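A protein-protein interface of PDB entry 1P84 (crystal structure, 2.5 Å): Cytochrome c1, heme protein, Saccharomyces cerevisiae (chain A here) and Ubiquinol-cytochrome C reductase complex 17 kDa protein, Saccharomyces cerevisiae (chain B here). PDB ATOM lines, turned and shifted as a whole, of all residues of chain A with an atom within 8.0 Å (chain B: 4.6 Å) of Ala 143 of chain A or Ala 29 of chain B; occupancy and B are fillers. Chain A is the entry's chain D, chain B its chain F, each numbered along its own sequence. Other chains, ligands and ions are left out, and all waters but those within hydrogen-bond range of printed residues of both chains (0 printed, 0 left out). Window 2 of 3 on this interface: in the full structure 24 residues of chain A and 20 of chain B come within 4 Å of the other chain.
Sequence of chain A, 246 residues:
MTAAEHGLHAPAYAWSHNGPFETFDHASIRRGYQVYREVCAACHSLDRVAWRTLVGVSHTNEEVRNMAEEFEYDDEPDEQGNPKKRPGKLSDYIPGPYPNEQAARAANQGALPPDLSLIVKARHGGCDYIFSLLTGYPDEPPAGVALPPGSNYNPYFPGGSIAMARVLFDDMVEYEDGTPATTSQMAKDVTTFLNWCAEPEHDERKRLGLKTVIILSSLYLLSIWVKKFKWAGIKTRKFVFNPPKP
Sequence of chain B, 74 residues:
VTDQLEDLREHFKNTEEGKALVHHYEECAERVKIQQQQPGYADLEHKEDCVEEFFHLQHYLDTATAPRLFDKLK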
ATOM      1  N   GLU A 140      -7.980 -13.825   2.092  1.00  0.00           N
ATOM      2  CA  GLU A 140      -9.314 -13.347   2.429  1.00  0.00           C
ATOM      3  C   GLU A 140      -9.311 -11.838   2.642  1.00  0.00           C
ATOM      4  O   GLU A 140      -8.368 -11.290   3.210  1.00  0.00           O
ATOM      5  CB  GLU A 140      -9.836 -14.056   3.683  1.00  0.00           C
ATOM      6  CG  GLU A 140     -10.271 -15.495   3.438  1.00  0.00           C
ATOM      7  CD  GLU A 140     -10.523 -16.264   4.722  1.00  0.00           C
ATOM      8  OE1 GLU A 140     -11.617 -16.102   5.310  1.00  0.00           O
ATOM      9  OE2 GLU A 140      -9.623 -17.034   5.137  1.00  0.00           O
ATOM     10  N   PRO A 141     -10.353 -11.144   2.150  1.00  0.00           N
ATOM     11  CA  PRO A 141     -10.468  -9.690   2.295  1.00  0.00           C
ATOM     12  C   PRO A 141     -10.645  -9.303   3.762  1.00  0.00           C
ATOM     13  O   PRO A 141     -11.099 -10.117   4.569  1.00  0.00           O
ATOM     14  CB  PRO A 141     -11.719  -9.368   1.476  1.00  0.00           C
ATOM     15  CG  PRO A 141     -12.534 -10.606   1.595  1.00  0.00           C
ATOM     16  CD  PRO A 141     -11.501 -11.681   1.400  1.00  0.00           C
ATOM     17  N   PRO A 142     -10.277  -8.064   4.131  1.00  0.00           N
ATOM     18  CA  PRO A 142     -10.424  -7.632   5.523  1.00  0.00           C
ATOM     19  C   PRO A 142     -11.890  -7.674   5.947  1.00  0.00           C
ATOM     20  O   PRO A 142     -12.792  -7.566   5.114  1.00  0.00           O
ATOM     21  CB  PRO A 142      -9.864  -6.207   5.498  1.00  0.00           C
ATOM     22  CG  PRO A 142     -10.159  -5.750   4.117  1.00  0.00           C
ATOM     23  CD  PRO A 142      -9.792  -6.955   3.291  1.00  0.00           C
ATOM     24  N   ALA A 143     -12.114  -7.858   7.244  1.00  0.00           N
ATOM     25  CA  ALA A 143     -13.463  -7.944   7.798  1.00  0.00           C
ATOM     26  C   ALA A 143     -14.338  -6.729   7.508  1.00  0.00           C
ATOM     27  O   ALA A 143     -13.918  -5.593   7.705  1.00  0.00           O
ATOM     28  CB  ALA A 143     -13.391  -8.193   9.300  1.00  0.00           C
ATOM     29  N   GLY A 144     -15.554  -6.983   7.034  1.00  0.00           N
ATOM     30  CA  GLY A 144     -16.482  -5.905   6.745  1.00  0.00           C
ATOM     31  C   GLY A 144     -16.579  -5.502   5.290  1.00  0.00           C
ATOM     32  O   GLY A 144     -17.548  -4.856   4.893  1.00  0.00           O
ATOM     33  N   VAL A 145     -15.584  -5.873   4.491  1.00  0.00           N
ATOM     34  CA  VAL A 145     -15.581  -5.527   3.075  1.00  0.00           C
ATOM     35  C   VAL A 145     -16.557  -6.370   2.258  1.00  0.00           C
ATOM     36  O   VAL A 145     -16.414  -7.592   2.153  1.00  0.00           O
ATOM     37  CB  VAL A 145     -14.163  -5.628   2.473  1.00  0.00           C
ATOM     38  CG1 VAL A 145     -14.199  -5.355   0.979  1.00  0.00           C
ATOM     39  CG2 VAL A 145     -13.248  -4.638   3.157  1.00  0.00           C
ATOM     40  N   ALA A 146     -17.560  -5.699   1.702  1.00  0.00           N
ATOM     41  CA  ALA A 146     -18.579  -6.344   0.881  1.00  0.00           C
ATOM     42  C   ALA A 146     -18.088  -6.402  -0.564  1.00  0.00           C
ATOM     43  O   ALA A 146     -18.420  -5.547  -1.391  1.00  0.00           O
ATOM     44  CB  ALA A 146     -19.890  -5.566   0.973  1.00  0.00           C
ATOM     45  N   TYR B  25      -6.198  -5.461  14.681  1.00  0.00           N
ATOM     46  CA  TYR B  25      -6.985  -5.843  13.517  1.00  0.00           C
ATOM     47  C   TYR B  25      -7.961  -6.934  13.925  1.00  0.00           C
ATOM     48  O   TYR B  25      -9.115  -6.944  13.489  1.00  0.00           O
ATOM     49  CB  TYR B  25      -6.100  -6.354  12.366  1.00  0.00           C
ATOM     50  CG  TYR B  25      -6.913  -7.044  11.287  1.00  0.00           C
ATOM     51  CD1 TYR B  25      -7.873  -6.342  10.565  1.00  0.00           C
ATOM     52  CD2 TYR B  25      -6.816  -8.421  11.080  1.00  0.00           C
ATOM     53  CE1 TYR B  25      -8.727  -6.988   9.677  1.00  0.00           C
ATOM     54  CE2 TYR B  25      -7.671  -9.077  10.190  1.00  0.00           C
ATOM     55  CZ  TYR B  25      -8.628  -8.350   9.498  1.00  0.00           C
ATOM     56  OH  TYR B  25      -9.518  -8.984   8.662  1.00  0.00           O
ATOM     57  N   GLU B  26      -7.475  -7.860  14.748  1.00  0.00           N
ATOM     58  CA  GLU B  26      -8.272  -8.984  15.236  1.00  0.00           C
ATOM     59  C   GLU B  26      -9.466  -8.479  16.030  1.00  0.00           C
ATOM     60  O   GLU B  26     -10.604  -8.890  15.791  1.00  0.00           O
ATOM     61  CB  GLU B  26      -7.412  -9.890  16.115  1.00  0.00           C
ATOM     62  CG  GLU B  26      -7.685 -11.359  15.919  1.00  0.00           C
ATOM     63  CD  GLU B  26      -7.468 -11.794  14.486  1.00  0.00           C
ATOM     64  OE1 GLU B  26      -8.431 -11.700  13.688  1.00  0.00           O
ATOM     65  OE2 GLU B  26      -6.336 -12.224  14.162  1.00  0.00           O
ATOM     66  N   GLU B  27      -9.191  -7.559  16.951  1.00  0.00           N
ATOM     67  CA  GLU B  27     -10.216  -6.959  17.788  1.00  0.00           C
ATOM     68  C   GLU B  27     -11.278  -6.283  16.918  1.00  0.00           C
ATOM     69  O   GLU B  27     -12.452  -6.221  17.299  1.00  0.00           O
ATOM     70  CB  GLU B  27      -9.579  -5.954  18.754  1.00  0.00           C
ATOM     71  CG  GLU B  27     -10.515  -5.460  19.855  1.00  0.00           C
ATOM     72  CD  GLU B  27      -9.778  -4.802  21.018  1.00  0.00           C
ATOM     73  OE1 GLU B  27      -9.784  -3.550  21.097  1.00  0.00           O
ATOM     74  OE2 GLU B  27      -9.202  -5.540  21.855  1.00  0.00           O
ATOM     75  N   CYS B  28     -10.871  -5.804  15.741  1.00  0.00           N
ATOM     76  CA  CYS B  28     -11.802  -5.161  14.821  1.00  0.00           C
ATOM     77  C   CYS B  28     -12.656  -6.207  14.118  1.00  0.00           C
ATOM     78  O   CYS B  28     -13.872  -6.071  14.061  1.00  0.00           O
ATOM     79  CB  CYS B  28     -11.066  -4.316  13.778  1.00  0.00           C
ATOM     80  SG  CYS B  28     -12.182  -3.422  12.631  1.00  0.00           S
ATOM     81  N   ALA B  29     -12.008  -7.241  13.583  1.00  0.00           N
ATOM     82  CA  ALA B  29     -12.695  -8.324  12.876  1.00  0.00           C
ATOM     83  C   ALA B  29     -13.763  -8.951  13.762  1.00  0.00           C
ATOM     84  O   ALA B  29     -14.875  -9.235  13.313  1.00  0.00           O
ATOM     85  CB  ALA B  29     -11.692  -9.378  12.447  1.00  0.00           C
ATOM     86  N   GLU B  30     -13.402  -9.150  15.028  1.00  0.00           N
ATOM     87  CA  GLU B  30     -14.287  -9.718  16.039  1.00  0.00           C
ATOM     88  C   GLU B  30     -15.523  -8.827  16.187  1.00  0.00           C
ATOM     89  O   GLU B  30     -16.650  -9.266  15.957  1.00  0.00           O
ATOM     90  CB  GLU B  30     -13.524  -9.812  17.365  1.00  0.00           C
ATOM     91  CG  GLU B  30     -14.291 -10.404  18.537  1.00  0.00           C
ATOM     92  CD  GLU B  30     -13.390 -10.658  19.738  1.00  0.00           C
ATOM     93  OE1 GLU B  30     -12.939  -9.678  20.381  1.00  0.00           O
ATOM     94  OE2 GLU B  30     -13.118 -11.844  20.029  1.00  0.00           O
ATOM     95  N   ARG B  31     -15.283  -7.560  16.508  1.00  0.00           N
ATOM     96  CA  ARG B  31     -16.336  -6.567  16.680  1.00  0.00           C
ATOM     97  C   ARG B  31     -17.270  -6.495  15.463  1.00  0.00           C
ATOM     98  O   ARG B  31     -18.460  -6.222  15.603  1.00  0.00           O
ATOM     99  CB  ARG B  31     -15.693  -5.200  16.945  1.00  0.00           C
ATOM    100  CG  ARG B  31     -16.665  -4.071  17.247  1.00  0.00           C
ATOM    101  CD  ARG B  31     -15.944  -2.811  17.728  1.00  0.00           C
ATOM    102  NE  ARG B  31     -15.087  -2.220  16.701  1.00  0.00           N
ATOM    103  CZ  ARG B  31     -13.759  -2.150  16.775  1.00  0.00           C
ATOM    104  NH1 ARG B  31     -13.066  -1.590  15.789  1.00  0.00           N
ATOM    105  NH2 ARG B  31     -13.118  -2.650  17.827  1.00  0.00           N
ATOM    106  N   VAL B  32     -16.733  -6.789  14.281  1.00  0.00           N
ATOM    107  CA  VAL B  32     -17.503  -6.741  13.040  1.00  0.00           C
ATOM    108  C   VAL B  32     -18.468  -7.905  12.825  1.00  0.00           C
ATOM    109  O   VAL B  32     -19.635  -7.680  12.507  1.00  0.00           O
ATOM    110  CB  VAL B  32     -16.578  -6.612  11.798  1.00  0.00           C
ATOM    111  CG1 VAL B  32     -17.397  -6.669  10.510  1.00  0.00           C
ATOM    112  CG2 VAL B  32     -15.808  -5.307  11.855  1.00  0.00           C
ATOM    113  N   LYS B  33     -17.990  -9.141  12.975  1.00  0.00           N
ATOM    114  CA  LYS B  33     -18.854 -10.309  12.773  1.00  0.00           C
ATOM    115  C   LYS B  33     -20.043 -10.330  13.735  1.00  0.00           C
ATOM    116  O   LYS B  33     -21.106 -10.856  13.408  1.00  0.00           O
ATOM    117  CB  LYS B  33     -18.066 -11.627  12.852  1.00  0.00           C
ATOM    118  CG  LYS B  33     -17.477 -11.978  14.214  1.00  0.00           C
ATOM    119  CD  LYS B  33     -16.918 -13.402  14.195  1.00  0.00           C
ATOM    120  CE  LYS B  33     -16.252 -13.793  15.512  1.00  0.00           C
ATOM    121  NZ  LYS B  33     -14.975 -13.056  15.747  1.00  0.00           N
ATOM    122  N   ASP B  49     -15.864  -1.485   8.699  1.00  0.00           N
ATOM    123  CA  ASP B  49     -14.941  -2.431   8.092  1.00  0.00           C
ATOM    124  C   ASP B  49     -13.608  -2.275   8.798  1.00  0.00           C
ATOM    125  O   ASP B  49     -13.418  -1.344   9.573  1.00  0.00           O
ATOM    126  CB  ASP B  49     -14.808  -2.236   6.572  1.00  0.00           C
ATOM    127  CG  ASP B  49     -14.397  -0.833   6.185  1.00  0.00           C
ATOM    128  OD1 ASP B  49     -15.168  -0.191   5.438  1.00  0.00           O
ATOM    129  OD2 ASP B  49     -13.303  -0.378   6.594  1.00  0.00           O
ATOM    130  N   CYS B  50     -12.688  -3.191   8.544  1.00  0.00           N
ATOM    131  CA  CYS B  50     -11.395  -3.140   9.200  1.00  0.00           C
ATOM    132  C   CYS B  50     -10.243  -2.836   8.257  1.00  0.00           C
ATOM    133  O   CYS B  50      -9.088  -3.161   8.544  1.00  0.00           O
ATOM    134  CB  CYS B  50     -11.171  -4.442   9.966  1.00  0.00           C
ATOM    135  SG  CYS B  50     -12.526  -4.763  11.144  1.00  0.00           S
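The backbone carbonyl oxygen (O) of Ala 143 of chain A sits at hydrogen-bond distance from the backbone NH (N) of Cys 50 of chain B. N of Ala 143 of chain A lies within hydrogen-bond range of OH of Tyr 25 of chain B, 3.2 Å away.
The side-chain sulfur (SG) of Cys 50 of chain B forms a disulfide with the side-chain sulfur (SG) of Cys 28 of chain B. N of Ala 29 of chain B lies within hydrogen-bond range of SG of Cys 50 of chain B (3.5 Å).
CA of Pro 142 of chain A touches OH of Tyr 25 of chain B (3.5 Å). Ala 143 of chain A touches Ala 29 of chain B. Ala 143 of chain A touches Asp 49 of chain B. Val 32 of chain B touches Gly 144 of chain A. Asp 49 of chain B touches Gly 144 of chain A.
Ala 143 of chain A touches four residues of chain B. Of the printed residues of chain B, Gly 144 of chain A touches Val 32 and Asp 49. Val 145 of chain A touches none of the printed residues of chain B. No residue of chain A comes within 4 Å of Cys 28 of chain B. Of the printed residues of chain A, Val 32 of chain B touches Gly 144 (3.9 Å). Of the printed residues of chain A, Asp 49 of chain B touches Ala 143 (3.3 Å) and Gly 144 (3.9 Å). The nearest residue of chain B that does not touch Ala 143 of chain A is Val 32 of chain B (4.3 Å). The nearest printed residue of chain B that does not touch Pro 142 of chain A is Cys 50 of chain B (4.4 Å).
Hydrophobic or aromatic side chains of chain B that line the printed part of chain A: Tyr 25, Ala 29 and Val 32. Of the 7 printed residues of chain A, 3 touch a printed residue of chain B. Along chain A the printed residues that touch a printed residue of chain B span positions 142 to 144. Among the printed residues, 7 pairs touch across the chains. Among the printed residues, no Asp or Glu carboxylate lies within 4 Å of a Lys or Arg side-chain nitrogen of the other chain.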
